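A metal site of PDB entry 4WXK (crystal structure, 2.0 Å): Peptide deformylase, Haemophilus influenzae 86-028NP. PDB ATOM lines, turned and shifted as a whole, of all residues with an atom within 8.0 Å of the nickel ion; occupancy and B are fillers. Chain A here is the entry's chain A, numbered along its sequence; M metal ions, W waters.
The nickel ion is bound by water W1 (2.1 Å), a ring nitrogen (NE2) of His 133 (2.1 Å), a ring nitrogen (NE2) of His 137 (2.1 Å) and the side-chain sulfur (SG) of Cys 91 (2.2 Å). The nickel ion has four donor atoms within binding distance.
Water W1 lies within hydrogen-bond range of OE2 of Glu 134 (2.5 Å) and OE1 of Gln 51 (2.7 Å).
The side-chain carboxylate (OE1) of Glu 134 sits at hydrogen-bond distance from the backbone NH (N) of Ala 48, at 3.2 Å. A ring nitrogen (NE2) of His 137 sits close to the side-chain amide oxygen (OE1) of Gln 51, 3.4 Å away. SG of Cys 91 sits close to N of Ser 93, at 3.6 Å. The side-chain amide oxygen of Gln 51 sits close to the side-chain carboxylate of Glu 134 (3.4 Å). The side-chain carboxylate (OE1) of Glu 89 lies within hydrogen-bond range of a ring nitrogen (ND1) of His 133 (2.7 Å). The side-chain amide nitrogen of Gln 51 lies within hydrogen-bond range of the side-chain hydroxyl of Ser 93 (3.0 Å). The side-chain amide nitrogen of Gln 51 lies close to the side-chain sulfur of Cys 91. The side-chain amide oxygen (OE1) of Gln 51 lies within hydrogen-bond range of the backbone NH (N) of Ala 48 (3.0 Å).
Merely in contact with the nickel ion: Gln 51 and Glu 134. Within 4 Å of the nickel ion: Gln 51, Cys 91, His 133, Glu 134 and His 137.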
ATOM      1  N   LEU A  14     -29.397  18.385   2.448  1.00  0.00           N
ATOM      2  CA  LEU A  14     -29.170  19.461   1.516  1.00  0.00           C
ATOM      3  C   LEU A  14     -29.727  20.815   2.043  1.00  0.00           C
ATOM      4  O   LEU A  14     -29.551  21.859   1.344  1.00  0.00           O
ATOM      5  CB  LEU A  14     -29.840  19.119   0.178  1.00  0.00           C
ATOM      6  CG  LEU A  14     -29.188  18.018  -0.628  1.00  0.00           C
ATOM      7  CD1 LEU A  14     -30.040  17.595  -1.824  1.00  0.00           C
ATOM      8  CD2 LEU A  14     -27.775  18.404  -1.025  1.00  0.00           C
ATOM      9  N   GLY A  46     -18.407  22.083  -9.642  1.00  0.00           N
ATOM     10  CA  GLY A  46     -18.359  22.349  -8.209  1.00  0.00           C
ATOM     11  C   GLY A  46     -19.067  21.266  -7.410  1.00  0.00           C
ATOM     12  O   GLY A  46     -19.981  20.597  -7.915  1.00  0.00           O
ATOM     13  N   LEU A  47     -18.613  21.064  -6.164  1.00  0.00           N
ATOM     14  CA  LEU A  47     -19.300  20.193  -5.241  1.00  0.00           C
ATOM     15  C   LEU A  47     -19.116  20.707  -3.854  1.00  0.00           C
ATOM     16  O   LEU A  47     -18.074  21.212  -3.543  1.00  0.00           O
ATOM     17  CB  LEU A  47     -18.774  18.774  -5.407  1.00  0.00           C
ATOM     18  CG  LEU A  47     -19.483  17.611  -4.761  1.00  0.00           C
ATOM     19  CD1 LEU A  47     -20.797  17.359  -5.470  1.00  0.00           C
ATOM     20  CD2 LEU A  47     -18.614  16.391  -4.930  1.00  0.00           C
ATOM     21  N   ALA A  48     -20.136  20.560  -3.011  1.00  0.00           N
ATOM     22  CA  ALA A  48     -20.025  20.856  -1.630  1.00  0.00           C
ATOM     23  C   ALA A  48     -20.299  19.581  -0.811  1.00  0.00           C
ATOM     24  O   ALA A  48     -21.098  18.756  -1.179  1.00  0.00           O
ATOM     25  CB  ALA A  48     -21.034  21.918  -1.297  1.00  0.00           C
ATOM     26  N   GLN A  51     -23.679  17.758  -0.252  1.00  0.00           N
ATOM     27  CA  GLN A  51     -24.161  16.969  -1.420  1.00  0.00           C
ATOM     28  C   GLN A  51     -23.726  15.559  -1.426  1.00  0.00           C
ATOM     29  O   GLN A  51     -24.274  14.770  -2.143  1.00  0.00           O
ATOM     30  CB  GLN A  51     -23.658  17.601  -2.701  1.00  0.00           C
ATOM     31  CG  GLN A  51     -24.226  18.985  -2.979  1.00  0.00           C
ATOM     32  CD  GLN A  51     -23.734  19.541  -4.296  1.00  0.00           C
ATOM     33  OE1 GLN A  51     -22.783  20.328  -4.344  1.00  0.00           O
ATOM     34  NE2 GLN A  51     -24.368  19.116  -5.382  1.00  0.00           N
ATOM     35  N   GLU A  89     -27.961  28.307 -13.827  1.00  0.00           N
ATOM     36  CA  GLU A  89     -27.159  27.387 -13.033  1.00  0.00           C
ATOM     37  C   GLU A  89     -27.818  26.051 -12.997  1.00  0.00           C
ATOM     38  O   GLU A  89     -29.072  25.937 -12.938  1.00  0.00           O
ATOM     39  CB  GLU A  89     -27.027  27.876 -11.555  1.00  0.00           C
ATOM     40  CG  GLU A  89     -26.214  29.152 -11.441  1.00  0.00           C
ATOM     41  CD  GLU A  89     -26.042  29.632 -10.030  1.00  0.00           C
ATOM     42  OE1 GLU A  89     -26.192  28.824  -9.088  1.00  0.00           O
ATOM     43  OE2 GLU A  89     -25.749  30.821  -9.842  1.00  0.00           O
ATOM     44  N   GLY A  90     -26.972  25.044 -13.037  1.00  0.00           N
ATOM     45  CA  GLY A  90     -27.361  23.690 -12.635  1.00  0.00           C
ATOM     46  C   GLY A  90     -26.618  23.194 -11.408  1.00  0.00           C
ATOM     47  O   GLY A  90     -25.829  23.927 -10.769  1.00  0.00           O
ATOM     48  N   CYS A  91     -26.838  21.925 -11.072  1.00  0.00           N
ATOM     49  CA  CYS A  91     -26.387  21.378  -9.796  1.00  0.00           C
ATOM     50  C   CYS A  91     -26.556  19.884  -9.846  1.00  0.00           C
ATOM     51  O   CYS A  91     -27.578  19.380 -10.311  1.00  0.00           O
ATOM     52  CB  CYS A  91     -27.184  21.939  -8.631  1.00  0.00           C
ATOM     53  SG  CYS A  91     -26.724  21.332  -6.968  1.00  0.00           S
ATOM     54  N   LEU A  92     -25.522  19.191  -9.480  1.00  0.00           N
ATOM     55  CA  LEU A  92     -25.525  17.723  -9.510  1.00  0.00           C
ATOM     56  C   LEU A  92     -26.603  17.131  -8.591  1.00  0.00           C
ATOM     57  O   LEU A  92     -27.101  16.046  -8.885  1.00  0.00           O
ATOM     58  CB  LEU A  92     -24.160  17.210  -9.064  1.00  0.00           C
ATOM     59  CG  LEU A  92     -23.002  17.490 -10.074  1.00  0.00           C
ATOM     60  CD1 LEU A  92     -21.746  16.848  -9.543  1.00  0.00           C
ATOM     61  CD2 LEU A  92     -23.359  16.879 -11.389  1.00  0.00           C
ATOM     62  N   SER A  93     -26.983  17.827  -7.503  1.00  0.00           N
ATOM     63  CA  SER A  93     -28.068  17.330  -6.650  1.00  0.00           C
ATOM     64  C   SER A  93     -29.426  17.671  -7.217  1.00  0.00           C
ATOM     65  O   SER A  93     -30.486  17.329  -6.607  1.00  0.00           O
ATOM     66  CB  SER A  93     -27.939  17.856  -5.239  1.00  0.00           C
ATOM     67  OG  SER A  93     -26.726  17.440  -4.700  1.00  0.00           O
ATOM     68  N   ILE A  94     -29.464  18.395  -8.337  1.00  0.00           N
ATOM     69  CA  ILE A  94     -30.728  18.771  -8.919  1.00  0.00           C
ATOM     70  C   ILE A  94     -30.686  18.490 -10.413  1.00  0.00           C
ATOM     71  O   ILE A  94     -30.810  19.385 -11.229  1.00  0.00           O
ATOM     72  CB  ILE A  94     -31.119  20.230  -8.626  1.00  0.00           C
ATOM     73  CG1 ILE A  94     -30.855  20.600  -7.155  1.00  0.00           C
ATOM     74  CG2 ILE A  94     -32.576  20.446  -8.992  1.00  0.00           C
ATOM     75  CD1 ILE A  94     -30.813  22.127  -6.873  1.00  0.00           C
ATOM     76  N   ARG A 103     -26.591  36.752  -8.924  1.00  0.00           N
ATOM     77  CA  ARG A 103     -25.377  36.612  -8.121  1.00  0.00           C
ATOM     78  C   ARG A 103     -24.571  37.898  -8.160  1.00  0.00           C
ATOM     79  O   ARG A 103     -24.781  38.784  -9.047  1.00  0.00           O
ATOM     80  CB  ARG A 103     -24.496  35.494  -8.728  1.00  0.00           C
ATOM     81  CG  ARG A 103     -25.087  34.053  -8.738  1.00  0.00           C
ATOM     82  CD  ARG A 103     -25.195  33.415  -7.370  1.00  0.00           C
ATOM     83  NE  ARG A 103     -25.646  31.994  -7.450  1.00  0.00           N
ATOM     84  CZ  ARG A 103     -26.047  31.302  -6.408  1.00  0.00           C
ATOM     85  NH1 ARG A 103     -26.052  31.863  -5.194  1.00  0.00           N
ATOM     86  NH2 ARG A 103     -26.480  30.070  -6.560  1.00  0.00           N
ATOM     87  N   CYS A 130     -19.716  30.084  -9.139  1.00  0.00           N
ATOM     88  CA  CYS A 130     -19.570  28.758  -8.554  1.00  0.00           C
ATOM     89  C   CYS A 130     -19.290  28.823  -7.113  1.00  0.00           C
ATOM     90  O   CYS A 130     -19.795  27.996  -6.383  1.00  0.00           O
ATOM     91  CB  CYS A 130     -18.420  27.996  -9.169  1.00  0.00           C
ATOM     92  SG  CYS A 130     -18.912  27.489 -10.804  1.00  0.00           S
ATOM     93  N   HIS A 133     -22.595  29.729  -5.353  1.00  0.00           N
ATOM     94  CA  HIS A 133     -23.425  28.532  -5.408  1.00  0.00           C
ATOM     95  C   HIS A 133     -23.023  27.518  -4.351  1.00  0.00           C
ATOM     96  O   HIS A 133     -23.879  26.975  -3.600  1.00  0.00           O
ATOM     97  CB  HIS A 133     -23.387  27.924  -6.845  1.00  0.00           C
ATOM     98  CG  HIS A 133     -24.169  26.656  -7.031  1.00  0.00           C
ATOM     99  ND1 HIS A 133     -25.263  26.578  -7.879  1.00  0.00           N
ATOM    100  CD2 HIS A 133     -23.969  25.410  -6.559  1.00  0.00           C
ATOM    101  CE1 HIS A 133     -25.722  25.328  -7.881  1.00  0.00           C
ATOM    102  NE2 HIS A 133     -24.960  24.602  -7.077  1.00  0.00           N
ATOM    103  N   GLU A 134     -21.748  27.203  -4.309  1.00  0.00           N
ATOM    104  CA  GLU A 134     -21.267  26.169  -3.428  1.00  0.00           C
ATOM    105  C   GLU A 134     -21.273  26.581  -1.955  1.00  0.00           C
ATOM    106  O   GLU A 134     -21.585  25.741  -1.065  1.00  0.00           O
ATOM    107  CB  GLU A 134     -19.875  25.695  -3.871  1.00  0.00           C
ATOM    108  CG  GLU A 134     -19.885  25.122  -5.260  1.00  0.00           C
ATOM    109  CD  GLU A 134     -20.790  23.931  -5.436  1.00  0.00           C
ATOM    110  OE1 GLU A 134     -21.072  23.280  -4.393  1.00  0.00           O
ATOM    111  OE2 GLU A 134     -21.202  23.657  -6.620  1.00  0.00           O
ATOM    112  N   ASP A 136     -23.570  28.518  -0.846  1.00  0.00           N
ATOM    113  CA  ASP A 136     -24.979  28.395  -0.526  1.00  0.00           C
ATOM    114  C   ASP A 136     -25.227  27.010   0.029  1.00  0.00           C
ATOM    115  O   ASP A 136     -25.935  26.892   1.033  1.00  0.00           O
ATOM    116  CB  ASP A 136     -25.907  28.674  -1.711  1.00  0.00           C
ATOM    117  CG  ASP A 136     -26.337  30.124  -1.817  1.00  0.00           C
ATOM    118  OD1 ASP A 136     -26.058  30.971  -0.921  1.00  0.00           O
ATOM    119  OD2 ASP A 136     -27.068  30.401  -2.772  1.00  0.00           O
ATOM    120  N   HIS A 137     -24.650  25.966  -0.604  1.00  0.00           N
ATOM    121  CA  HIS A 137     -24.814  24.590  -0.097  1.00  0.00           C
ATOM    122  C   HIS A 137     -24.426  24.419   1.383  1.00  0.00           C
ATOM    123  O   HIS A 137     -25.103  23.678   2.128  1.00  0.00           O
ATOM    124  CB  HIS A 137     -24.026  23.581  -0.881  1.00  0.00           C
ATOM    125  CG  HIS A 137     -24.648  23.203  -2.190  1.00  0.00           C
ATOM    126  ND1 HIS A 137     -25.908  22.638  -2.298  1.00  0.00           N
ATOM    127  CD2 HIS A 137     -24.168  23.277  -3.446  1.00  0.00           C
ATOM    128  CE1 HIS A 137     -26.168  22.376  -3.562  1.00  0.00           C
ATOM    129  NE2 HIS A 137     -25.136  22.776  -4.286  1.00  0.00           N
ATOM    130  N   ILE A 141     -28.681  26.038   1.308  1.00  0.00           N
ATOM    131  CA  ILE A 141     -29.443  26.777   0.263  1.00  0.00           C
ATOM    132  C   ILE A 141     -29.131  26.207  -1.152  1.00  0.00           C
ATOM    133  O   ILE A 141     -27.976  25.978  -1.522  1.00  0.00           O
ATOM    134  CB  ILE A 141     -29.098  28.261   0.356  1.00  0.00           C
ATOM    135  CG1 ILE A 141     -29.574  28.831   1.719  1.00  0.00           C
ATOM    136  CG2 ILE A 141     -29.758  29.044  -0.772  1.00  0.00           C
ATOM    137  CD1 ILE A 141     -29.164  30.284   1.901  1.00  0.00           C
ATOM    138  N   LEU A 142     -30.183  26.008  -1.929  1.00  0.00           N
ATOM    139  CA  LEU A 142     -30.098  25.445  -3.260  1.00  0.00           C
ATOM    140  C   LEU A 142     -30.627  26.455  -4.255  1.00  0.00           C
ATOM    141  O   LEU A 142     -31.399  27.376  -3.882  1.00  0.00           O
ATOM    142  CB  LEU A 142     -31.011  24.183  -3.344  1.00  0.00           C
ATOM    143  CG  LEU A 142     -30.702  23.156  -2.236  1.00  0.00           C
ATOM    144  CD1 LEU A 142     -31.751  22.085  -2.295  1.00  0.00           C
ATOM    145  CD2 LEU A 142     -29.343  22.505  -2.416  1.00  0.00           C
ATOM    146  N   PHE A 143     -30.311  26.220  -5.535  1.00  0.00           N
ATOM    147  CA  PHE A 143     -30.669  27.227  -6.499  1.00  0.00           C
ATOM    148  C   PHE A 143     -32.177  27.322  -6.621  1.00  0.00           C
ATOM    149  O   PHE A 143     -32.726  28.386  -6.902  1.00  0.00           O
ATOM    150  CB  PHE A 143     -29.930  27.122  -7.845  1.00  0.00           C
ATOM    151  CG  PHE A 143     -30.399  26.022  -8.728  1.00  0.00           C
ATOM    152  CD1 PHE A 143     -31.598  26.138  -9.482  1.00  0.00           C
ATOM    153  CD2 PHE A 143     -29.638  24.904  -8.910  1.00  0.00           C
ATOM    154  CE1 PHE A 143     -31.991  25.153 -10.354  1.00  0.00           C
ATOM    155  CE2 PHE A 143     -30.014  23.925  -9.797  1.00  0.00           C
ATOM    156  CZ  PHE A 143     -31.194  24.028 -10.505  1.00  0.00           C
HETATM  157 NI    NI M   1     -25.035  22.657  -6.384  1.00  0.00          NI
HETATM  158  O   HOH W   1     -23.080  22.038  -6.402  1.00  0.00           O
HETATM  159  O   HOH W   2     -28.085  24.149  -5.596  1.00  0.00           O
